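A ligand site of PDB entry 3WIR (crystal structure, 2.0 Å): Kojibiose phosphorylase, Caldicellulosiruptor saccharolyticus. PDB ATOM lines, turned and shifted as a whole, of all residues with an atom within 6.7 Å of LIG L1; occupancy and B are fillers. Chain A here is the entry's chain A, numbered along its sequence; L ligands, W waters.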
ATOM      1  N   ALA A 329      19.098 -10.689 -12.166  1.00  0.00           N
ATOM      2  CA  ALA A 329      17.798 -11.037 -12.731  1.00  0.00           C
ATOM      3  C   ALA A 329      17.703 -10.609 -14.160  1.00  0.00           C
ATOM      4  O   ALA A 329      16.849 -11.087 -14.854  1.00  0.00           O
ATOM      5  CB  ALA A 329      16.706 -10.368 -11.932  1.00  0.00           C
ATOM      6  N   LYS A 330      18.568  -9.683 -14.606  1.00  0.00           N
ATOM      7  CA  LYS A 330      18.515  -9.233 -15.978  1.00  0.00           C
ATOM      8  C   LYS A 330      19.873  -9.422 -16.609  1.00  0.00           C
ATOM      9  O   LYS A 330      20.321  -8.599 -17.436  1.00  0.00           O
ATOM     10  CB  LYS A 330      18.189  -7.755 -16.091  1.00  0.00           C
ATOM     11  CG  LYS A 330      16.908  -7.271 -15.396  1.00  0.00           C
ATOM     12  CD  LYS A 330      15.678  -7.530 -16.206  1.00  0.00           C
ATOM     13  CE  LYS A 330      14.417  -6.918 -15.587  1.00  0.00           C
ATOM     14  NZ  LYS A 330      13.361  -7.862 -15.848  1.00  0.00           N
ATOM     15  N   TYR A 337      16.265  -4.036 -12.008  1.00  0.00           N
ATOM     16  CA  TYR A 337      16.545  -4.733 -10.695  1.00  0.00           C
ATOM     17  C   TYR A 337      18.008  -4.562 -10.225  1.00  0.00           C
ATOM     18  O   TYR A 337      18.479  -5.289  -9.342  1.00  0.00           O
ATOM     19  CB  TYR A 337      16.142  -6.224 -10.683  1.00  0.00           C
ATOM     20  CG  TYR A 337      14.652  -6.542 -10.869  1.00  0.00           C
ATOM     21  CD1 TYR A 337      13.673  -5.918 -10.087  1.00  0.00           C
ATOM     22  CD2 TYR A 337      14.210  -7.460 -11.828  1.00  0.00           C
ATOM     23  CE1 TYR A 337      12.296  -6.178 -10.239  1.00  0.00           C
ATOM     24  CE2 TYR A 337      12.833  -7.736 -11.980  1.00  0.00           C
ATOM     25  CZ  TYR A 337      11.882  -7.067 -11.181  1.00  0.00           C
ATOM     26  OH  TYR A 337      10.554  -7.297 -11.305  1.00  0.00           O
ATOM     27  N   PHE A 342      18.681 -13.008  -7.356  1.00  0.00           N
ATOM     28  CA  PHE A 342      17.447 -13.516  -6.702  1.00  0.00           C
ATOM     29  C   PHE A 342      17.362 -15.045  -6.883  1.00  0.00           C
ATOM     30  O   PHE A 342      18.178 -15.676  -7.587  1.00  0.00           O
ATOM     31  CB  PHE A 342      16.192 -12.962  -7.394  1.00  0.00           C
ATOM     32  CG  PHE A 342      16.029 -11.467  -7.422  1.00  0.00           C
ATOM     33  CD1 PHE A 342      14.903 -10.912  -6.849  1.00  0.00           C
ATOM     34  CD2 PHE A 342      16.866 -10.619  -8.228  1.00  0.00           C
ATOM     35  CE1 PHE A 342      14.641  -9.567  -6.919  1.00  0.00           C
ATOM     36  CE2 PHE A 342      16.612  -9.268  -8.326  1.00  0.00           C
ATOM     37  CZ  PHE A 342      15.492  -8.719  -7.675  1.00  0.00           C
ATOM     38  N   TRP A 343      16.355 -15.656  -6.279  1.00  0.00           N
ATOM     39  CA  TRP A 343      16.029 -17.064  -6.556  1.00  0.00           C
ATOM     40  C   TRP A 343      15.938 -17.449  -8.066  1.00  0.00           C
ATOM     41  O   TRP A 343      16.092 -18.629  -8.440  1.00  0.00           O
ATOM     42  CB  TRP A 343      14.745 -17.486  -5.816  1.00  0.00           C
ATOM     43  CG  TRP A 343      13.427 -17.147  -6.457  1.00  0.00           C
ATOM     44  CD1 TRP A 343      12.997 -15.915  -6.887  1.00  0.00           C
ATOM     45  CD2 TRP A 343      12.265 -18.018  -6.549  1.00  0.00           C
ATOM     46  NE1 TRP A 343      11.717 -16.015  -7.381  1.00  0.00           N
ATOM     47  CE2 TRP A 343      11.236 -17.278  -7.150  1.00  0.00           C
ATOM     48  CE3 TRP A 343      12.046 -19.367  -6.234  1.00  0.00           C
ATOM     49  CZ2 TRP A 343       9.972 -17.831  -7.403  1.00  0.00           C
ATOM     50  CZ3 TRP A 343      10.789 -19.930  -6.540  1.00  0.00           C
ATOM     51  CH2 TRP A 343       9.774 -19.151  -7.108  1.00  0.00           C
ATOM     52  N   ASP A 344      15.671 -16.479  -8.911  1.00  0.00           N
ATOM     53  CA  ASP A 344      15.763 -16.628 -10.378  1.00  0.00           C
ATOM     54  C   ASP A 344      16.982 -17.449 -10.851  1.00  0.00           C
ATOM     55  O   ASP A 344      16.930 -18.342 -11.741  1.00  0.00           O
ATOM     56  CB  ASP A 344      15.925 -15.242 -10.962  1.00  0.00           C
ATOM     57  CG  ASP A 344      14.711 -14.332 -10.745  1.00  0.00           C
ATOM     58  OD1 ASP A 344      14.439 -13.678 -11.735  1.00  0.00           O
ATOM     59  OD2 ASP A 344      14.125 -14.235  -9.621  1.00  0.00           O
ATOM     60  N   PHE A 348      15.614 -21.064 -11.486  1.00  0.00           N
ATOM     61  CA  PHE A 348      15.315 -20.950 -12.905  1.00  0.00           C
ATOM     62  C   PHE A 348      16.475 -21.167 -13.847  1.00  0.00           C
ATOM     63  O   PHE A 348      16.415 -21.943 -14.854  1.00  0.00           O
ATOM     64  CB  PHE A 348      14.601 -19.606 -13.171  1.00  0.00           C
ATOM     65  CG  PHE A 348      13.187 -19.565 -12.630  1.00  0.00           C
ATOM     66  CD1 PHE A 348      12.078 -19.852 -13.469  1.00  0.00           C
ATOM     67  CD2 PHE A 348      12.975 -19.324 -11.264  1.00  0.00           C
ATOM     68  CE1 PHE A 348      10.784 -19.892 -12.958  1.00  0.00           C
ATOM     69  CE2 PHE A 348      11.682 -19.375 -10.745  1.00  0.00           C
ATOM     70  CZ  PHE A 348      10.593 -19.679 -11.596  1.00  0.00           C
ATOM     71  N   TRP A 391      16.835 -11.661   0.043  1.00  0.00           N
ATOM     72  CA  TRP A 391      15.993 -11.793  -1.121  1.00  0.00           C
ATOM     73  C   TRP A 391      16.711 -11.288  -2.407  1.00  0.00           C
ATOM     74  O   TRP A 391      16.572 -11.868  -3.466  1.00  0.00           O
ATOM     75  CB  TRP A 391      14.695 -11.022  -0.905  1.00  0.00           C
ATOM     76  CG  TRP A 391      13.804 -11.131  -2.147  1.00  0.00           C
ATOM     77  CD1 TRP A 391      13.431 -10.156  -2.946  1.00  0.00           C
ATOM     78  CD2 TRP A 391      13.208 -12.319  -2.650  1.00  0.00           C
ATOM     79  NE1 TRP A 391      12.641 -10.636  -3.979  1.00  0.00           N
ATOM     80  CE2 TRP A 391      12.485 -11.972  -3.806  1.00  0.00           C
ATOM     81  CE3 TRP A 391      13.194 -13.639  -2.233  1.00  0.00           C
ATOM     82  CZ2 TRP A 391      11.845 -12.875  -4.569  1.00  0.00           C
ATOM     83  CZ3 TRP A 391      12.540 -14.554  -3.012  1.00  0.00           C
ATOM     84  CH2 TRP A 391      11.880 -14.160  -4.188  1.00  0.00           C
ATOM     85  N   GLU A 421       9.868 -12.327   2.312  1.00  0.00           N
ATOM     86  CA  GLU A 421       9.914 -13.398   1.291  1.00  0.00           C
ATOM     87  C   GLU A 421      11.079 -14.336   1.592  1.00  0.00           C
ATOM     88  O   GLU A 421      12.195 -14.210   1.020  1.00  0.00           O
ATOM     89  CB  GLU A 421      10.003 -12.853  -0.146  1.00  0.00           C
ATOM     90  CG  GLU A 421       9.618 -13.909  -1.155  1.00  0.00           C
ATOM     91  CD  GLU A 421       9.247 -13.390  -2.563  1.00  0.00           C
ATOM     92  OE1 GLU A 421       9.354 -12.181  -2.854  1.00  0.00           O
ATOM     93  OE2 GLU A 421       8.791 -14.240  -3.350  1.00  0.00           O
ATOM     94  N   HIS A 423      11.618 -17.593   1.334  1.00  0.00           N
ATOM     95  CA  HIS A 423      11.843 -18.886   0.747  1.00  0.00           C
ATOM     96  C   HIS A 423      13.187 -18.988   0.019  1.00  0.00           C
ATOM     97  O   HIS A 423      13.736 -20.076  -0.126  1.00  0.00           O
ATOM     98  CB  HIS A 423      10.629 -19.323  -0.121  1.00  0.00           C
ATOM     99  CG  HIS A 423      10.326 -18.425  -1.281  1.00  0.00           C
ATOM    100  ND1 HIS A 423      10.962 -18.550  -2.507  1.00  0.00           N
ATOM    101  CD2 HIS A 423       9.494 -17.372  -1.405  1.00  0.00           C
ATOM    102  CE1 HIS A 423      10.512 -17.633  -3.327  1.00  0.00           C
ATOM    103  NE2 HIS A 423       9.632 -16.898  -2.683  1.00  0.00           N
ATOM    104  N   PRO A 481       6.091 -17.296  -3.415  1.00  0.00           N
ATOM    105  CA  PRO A 481       6.378 -17.045  -4.830  1.00  0.00           C
ATOM    106  C   PRO A 481       5.341 -16.179  -5.483  1.00  0.00           C
ATOM    107  O   PRO A 481       5.690 -15.327  -6.268  1.00  0.00           O
ATOM    108  CB  PRO A 481       6.427 -18.449  -5.438  1.00  0.00           C
ATOM    109  CG  PRO A 481       6.934 -19.287  -4.331  1.00  0.00           C
ATOM    110  CD  PRO A 481       6.239 -18.718  -3.109  1.00  0.00           C
ATOM    111  N   ASP A 482       4.083 -16.315  -5.099  1.00  0.00           N
ATOM    112  CA  ASP A 482       3.103 -15.369  -5.588  1.00  0.00           C
ATOM    113  C   ASP A 482       3.118 -14.129  -4.757  1.00  0.00           C
ATOM    114  O   ASP A 482       2.489 -14.072  -3.690  1.00  0.00           O
ATOM    115  CB  ASP A 482       1.705 -15.964  -5.641  1.00  0.00           C
ATOM    116  CG  ASP A 482       0.632 -14.901  -5.701  1.00  0.00           C
ATOM    117  OD1 ASP A 482       0.839 -13.912  -6.435  1.00  0.00           O
ATOM    118  OD2 ASP A 482      -0.434 -15.079  -5.044  1.00  0.00           O
ATOM    119  N   GLU A 483       3.742 -13.076  -5.291  1.00  0.00           N
ATOM    120  CA  GLU A 483       3.977 -11.858  -4.529  1.00  0.00           C
ATOM    121  C   GLU A 483       2.728 -10.952  -4.480  1.00  0.00           C
ATOM    122  O   GLU A 483       2.738  -9.953  -3.785  1.00  0.00           O
ATOM    123  CB  GLU A 483       5.182 -11.073  -5.107  1.00  0.00           C
ATOM    124  CG  GLU A 483       6.571 -11.703  -4.861  1.00  0.00           C
ATOM    125  CD  GLU A 483       7.726 -10.844  -5.418  1.00  0.00           C
ATOM    126  OE1 GLU A 483       8.894 -11.119  -5.017  1.00  0.00           O
ATOM    127  OE2 GLU A 483       7.445  -9.897  -6.222  1.00  0.00           O
ATOM    128  N   LYS A 596       0.202 -14.272  -9.255  1.00  0.00           N
ATOM    129  CA  LYS A 596       1.181 -13.612 -10.136  1.00  0.00           C
ATOM    130  C   LYS A 596       1.872 -14.635 -10.982  1.00  0.00           C
ATOM    131  O   LYS A 596       2.145 -14.387 -12.152  1.00  0.00           O
ATOM    132  CB  LYS A 596       2.203 -12.853  -9.285  1.00  0.00           C
ATOM    133  CG  LYS A 596       3.217 -11.998 -10.070  1.00  0.00           C
ATOM    134  CD  LYS A 596       4.098 -11.194  -9.105  1.00  0.00           C
ATOM    135  CE  LYS A 596       5.083 -10.304  -9.890  1.00  0.00           C
ATOM    136  NZ  LYS A 596       6.000  -9.772  -8.881  1.00  0.00           N
ATOM    137  N   GLN A 597       2.182 -15.748 -10.367  1.00  0.00           N
ATOM    138  CA  GLN A 597       3.021 -16.784 -10.924  1.00  0.00           C
ATOM    139  C   GLN A 597       2.759 -18.056 -10.151  1.00  0.00           C
ATOM    140  O   GLN A 597       2.024 -18.034  -9.146  1.00  0.00           O
ATOM    141  CB  GLN A 597       4.511 -16.408 -10.755  1.00  0.00           C
ATOM    142  CG  GLN A 597       4.920 -15.974  -9.339  1.00  0.00           C
ATOM    143  CD  GLN A 597       6.160 -15.102  -9.357  1.00  0.00           C
ATOM    144  OE1 GLN A 597       6.105 -13.879  -9.268  1.00  0.00           O
ATOM    145  NE2 GLN A 597       7.281 -15.737  -9.363  1.00  0.00           N
ATOM    146  N   LYS A 630       1.964 -12.422 -14.405  1.00  0.00           N
ATOM    147  CA  LYS A 630       2.516 -11.081 -14.275  1.00  0.00           C
ATOM    148  C   LYS A 630       3.987 -11.061 -13.835  1.00  0.00           C
ATOM    149  O   LYS A 630       4.499 -10.063 -13.357  1.00  0.00           O
ATOM    150  CB  LYS A 630       1.643 -10.216 -13.356  1.00  0.00           C
ATOM    151  CG  LYS A 630       0.381  -9.679 -14.061  1.00  0.00           C
ATOM    152  CD  LYS A 630       0.671  -8.401 -14.826  1.00  0.00           C
ATOM    153  CE  LYS A 630      -0.406  -8.155 -15.852  1.00  0.00           C
ATOM    154  NZ  LYS A 630       0.020  -7.128 -16.819  1.00  0.00           N
ATOM    155  N   SER A 631       4.643 -12.188 -14.001  1.00  0.00           N
ATOM    156  CA  SER A 631       6.079 -12.268 -13.892  1.00  0.00           C
ATOM    157  C   SER A 631       6.479 -13.145 -15.035  1.00  0.00           C
ATOM    158  O   SER A 631       5.797 -14.098 -15.398  1.00  0.00           O
ATOM    159  CB  SER A 631       6.501 -12.901 -12.538  1.00  0.00           C
ATOM    160  OG  SER A 631       7.811 -13.409 -12.548  1.00  0.00           O
ATOM    161  N   SER A 632       7.594 -12.788 -15.621  1.00  0.00           N
ATOM    162  CA  SER A 632       8.148 -13.574 -16.632  1.00  0.00           C
ATOM    163  C   SER A 632       8.615 -14.961 -16.167  1.00  0.00           C
ATOM    164  O   SER A 632       8.866 -15.778 -16.987  1.00  0.00           O
ATOM    165  CB  SER A 632       9.353 -12.789 -17.259  1.00  0.00           C
ATOM    166  OG  SER A 632      10.308 -12.723 -16.267  1.00  0.00           O
ATOM    167  N   LEU A 633       8.695 -15.243 -14.851  1.00  0.00           N
ATOM    168  CA  LEU A 633       9.000 -16.615 -14.324  1.00  0.00           C
ATOM    169  C   LEU A 633       7.788 -17.526 -14.462  1.00  0.00           C
ATOM    170  O   LEU A 633       7.942 -18.739 -14.362  1.00  0.00           O
ATOM    171  CB  LEU A 633       9.347 -16.563 -12.826  1.00  0.00           C
ATOM    172  CG  LEU A 633      10.730 -16.011 -12.414  1.00  0.00           C
ATOM    173  CD1 LEU A 633      11.027 -14.659 -13.010  1.00  0.00           C
ATOM    174  CD2 LEU A 633      10.929 -15.925 -10.902  1.00  0.00           C
ATOM    175  N   ALA A 677      15.723 -15.259 -15.771  1.00  0.00           N
ATOM    176  CA  ALA A 677      15.001 -16.438 -15.319  1.00  0.00           C
ATOM    177  C   ALA A 677      14.233 -17.165 -16.448  1.00  0.00           C
ATOM    178  O   ALA A 677      14.345 -18.376 -16.569  1.00  0.00           O
ATOM    179  CB  ALA A 677      14.024 -16.066 -14.229  1.00  0.00           C
HETATM  180  C1  LIG L   1       8.973 -11.867  -9.233  1.00  0.00           C
HETATM  181  C2  LIG L   1       9.974 -12.545  -8.345  1.00  0.00           C
HETATM  182  C3  LIG L   1      11.337 -12.423  -9.084  1.00  0.00           C
HETATM  183  C4  LIG L   1      11.790 -10.992  -9.346  1.00  0.00           C
HETATM  184  C5  LIG L   1      13.097 -10.915 -10.126  1.00  0.00           C
HETATM  185  C6  LIG L   1       9.411 -10.443  -9.453  1.00  0.00           C
HETATM  186  O1  LIG L   1       8.432  -9.874 -10.289  1.00  0.00           O
HETATM  187  O2  LIG L   1       7.630 -11.878  -8.742  1.00  0.00           O
HETATM  188  O3  LIG L   1       9.762 -13.968  -8.223  1.00  0.00           O
HETATM  189  O4  LIG L   1      12.282 -13.095  -8.262  1.00  0.00           O
HETATM  190  O5  LIG L   1      10.733 -10.356 -10.070  1.00  0.00           O
HETATM  191  O6  LIG L   1      12.964 -11.337 -11.489  1.00  0.00           O
HETATM  192  C1  LG2 L   2       9.766  -7.527  -7.289  1.00  0.00           C
HETATM  193  C2  LG2 L   2      10.357  -8.043  -5.967  1.00  0.00           C
HETATM  194  C3  LG2 L   2      11.590  -7.180  -5.638  1.00  0.00           C
HETATM  195  C4  LG2 L   2      11.137  -5.704  -5.678  1.00  0.00           C
HETATM  196  C5  LG2 L   2      12.250  -4.714  -5.376  1.00  0.00           C
HETATM  197  C6  LG2 L   2       9.504  -6.044  -7.333  1.00  0.00           C
HETATM  198  O1  LG2 L   2       9.155  -5.774  -8.690  1.00  0.00           O
HETATM  199  O2  LG2 L   2       8.460  -8.039  -7.582  1.00  0.00           O
HETATM  200  O3  LG2 L   2      10.590  -9.456  -6.118  1.00  0.00           O
HETATM  201  O4  LG2 L   2      12.165  -7.350  -4.337  1.00  0.00           O
HETATM  202  O5  LG2 L   2      10.632  -5.279  -6.960  1.00  0.00           O
HETATM  203  O6  LG2 L   2      13.353  -4.972  -6.253  1.00  0.00           O
HETATM  204  O   HOH W   1       8.388 -14.738  -6.134  1.00  0.00           O
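OE2 of Glu 483 sits at hydrogen-bond distance from O2 of LIG L1. OE2 of Glu 483 is in hydrogen-bond range of O2 of LG2 L2 (2.5 Å). OH of Tyr 337 sits at hydrogen-bond distance from O5 of LIG L1 (3.3 Å). The side-chain amino group (NZ) of Lys 596 lies within hydrogen-bond range of an oxygen (O2) of LIG L1 (2.7 Å). The indole nitrogen of Trp 391 sits at hydrogen-bond distance from an oxygen (O3) of LG2 L2 (3.2 Å). NE1 of Trp 343 lies within hydrogen-bond range of O3 of LIG L1. The side-chain hydroxyl of Tyr 337 is in hydrogen-bond range of an oxygen (O1) of LG2 L2, 3.3 Å away. An oxygen (O2) of LIG L1 is in hydrogen-bond range of the side-chain amide oxygen (OE1) of Gln 597, at 2.6 Å. The side-chain amino group (NZ) of Lys 596 lies within hydrogen-bond range of an oxygen (O2) of LG2 L2 (3.3 Å). OD2 of Asp 344 sits at hydrogen-bond distance from O4 of LIG L1, 2.6 Å away.
An oxygen (O1) of LIG L1 sits close to an oxygen (O2) of LG2 L2 (3.3 Å).
The side-chain carboxylate (OE1) of Glu 483 lies close to the side-chain carboxylate (OE1) of Glu 421 (2.5 Å). NZ of Lys 596 is in salt-bridge range of OE2 of Glu 483. The backbone NH (N) of Lys 596 is in hydrogen-bond range of the side-chain carboxylate (OD1) of Asp 482 (2.9 Å). The side-chain hydroxyl (OG) of Ser 631 sits close to the backbone NH (N) of Leu 633, 3.1 Å away. The backbone NH of Lys 630 is in hydrogen-bond range of the backbone carbonyl oxygen of Lys 596 (3.0 Å). OE1 of Gln 597 sits close to O of Pro 481 (3.4 Å).
CB of Ala 329 touches O6 of LIG L1 (3.9 Å). CD1 of Phe 342 touches O4 of LIG L1, 3.7 Å away. Trp 391 touches LIG L1. Ser 631 touches LIG L1. Leu 633 touches LIG L1. Hydrophobic or aromatic side chains that line LIG L1: Ala 329, Tyr 337, Phe 342, Trp 343, Trp 391 and Leu 633. 11 residues have an atom within 4 Å of LIG L1: Ala 329, Tyr 337, Phe 342, Trp 343, Asp 344, Trp 391, Glu 483, Lys 596, Gln 597, Ser 631 and Leu 633.
Water W1 lies within hydrogen-bond range of an oxygen (O3) of LIG L1 (2.6 Å), the backbone carbonyl oxygen (O) of Pro 481 (2.8 Å) and the side-chain carboxylate (OE2) of Glu 421 (2.9 Å).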
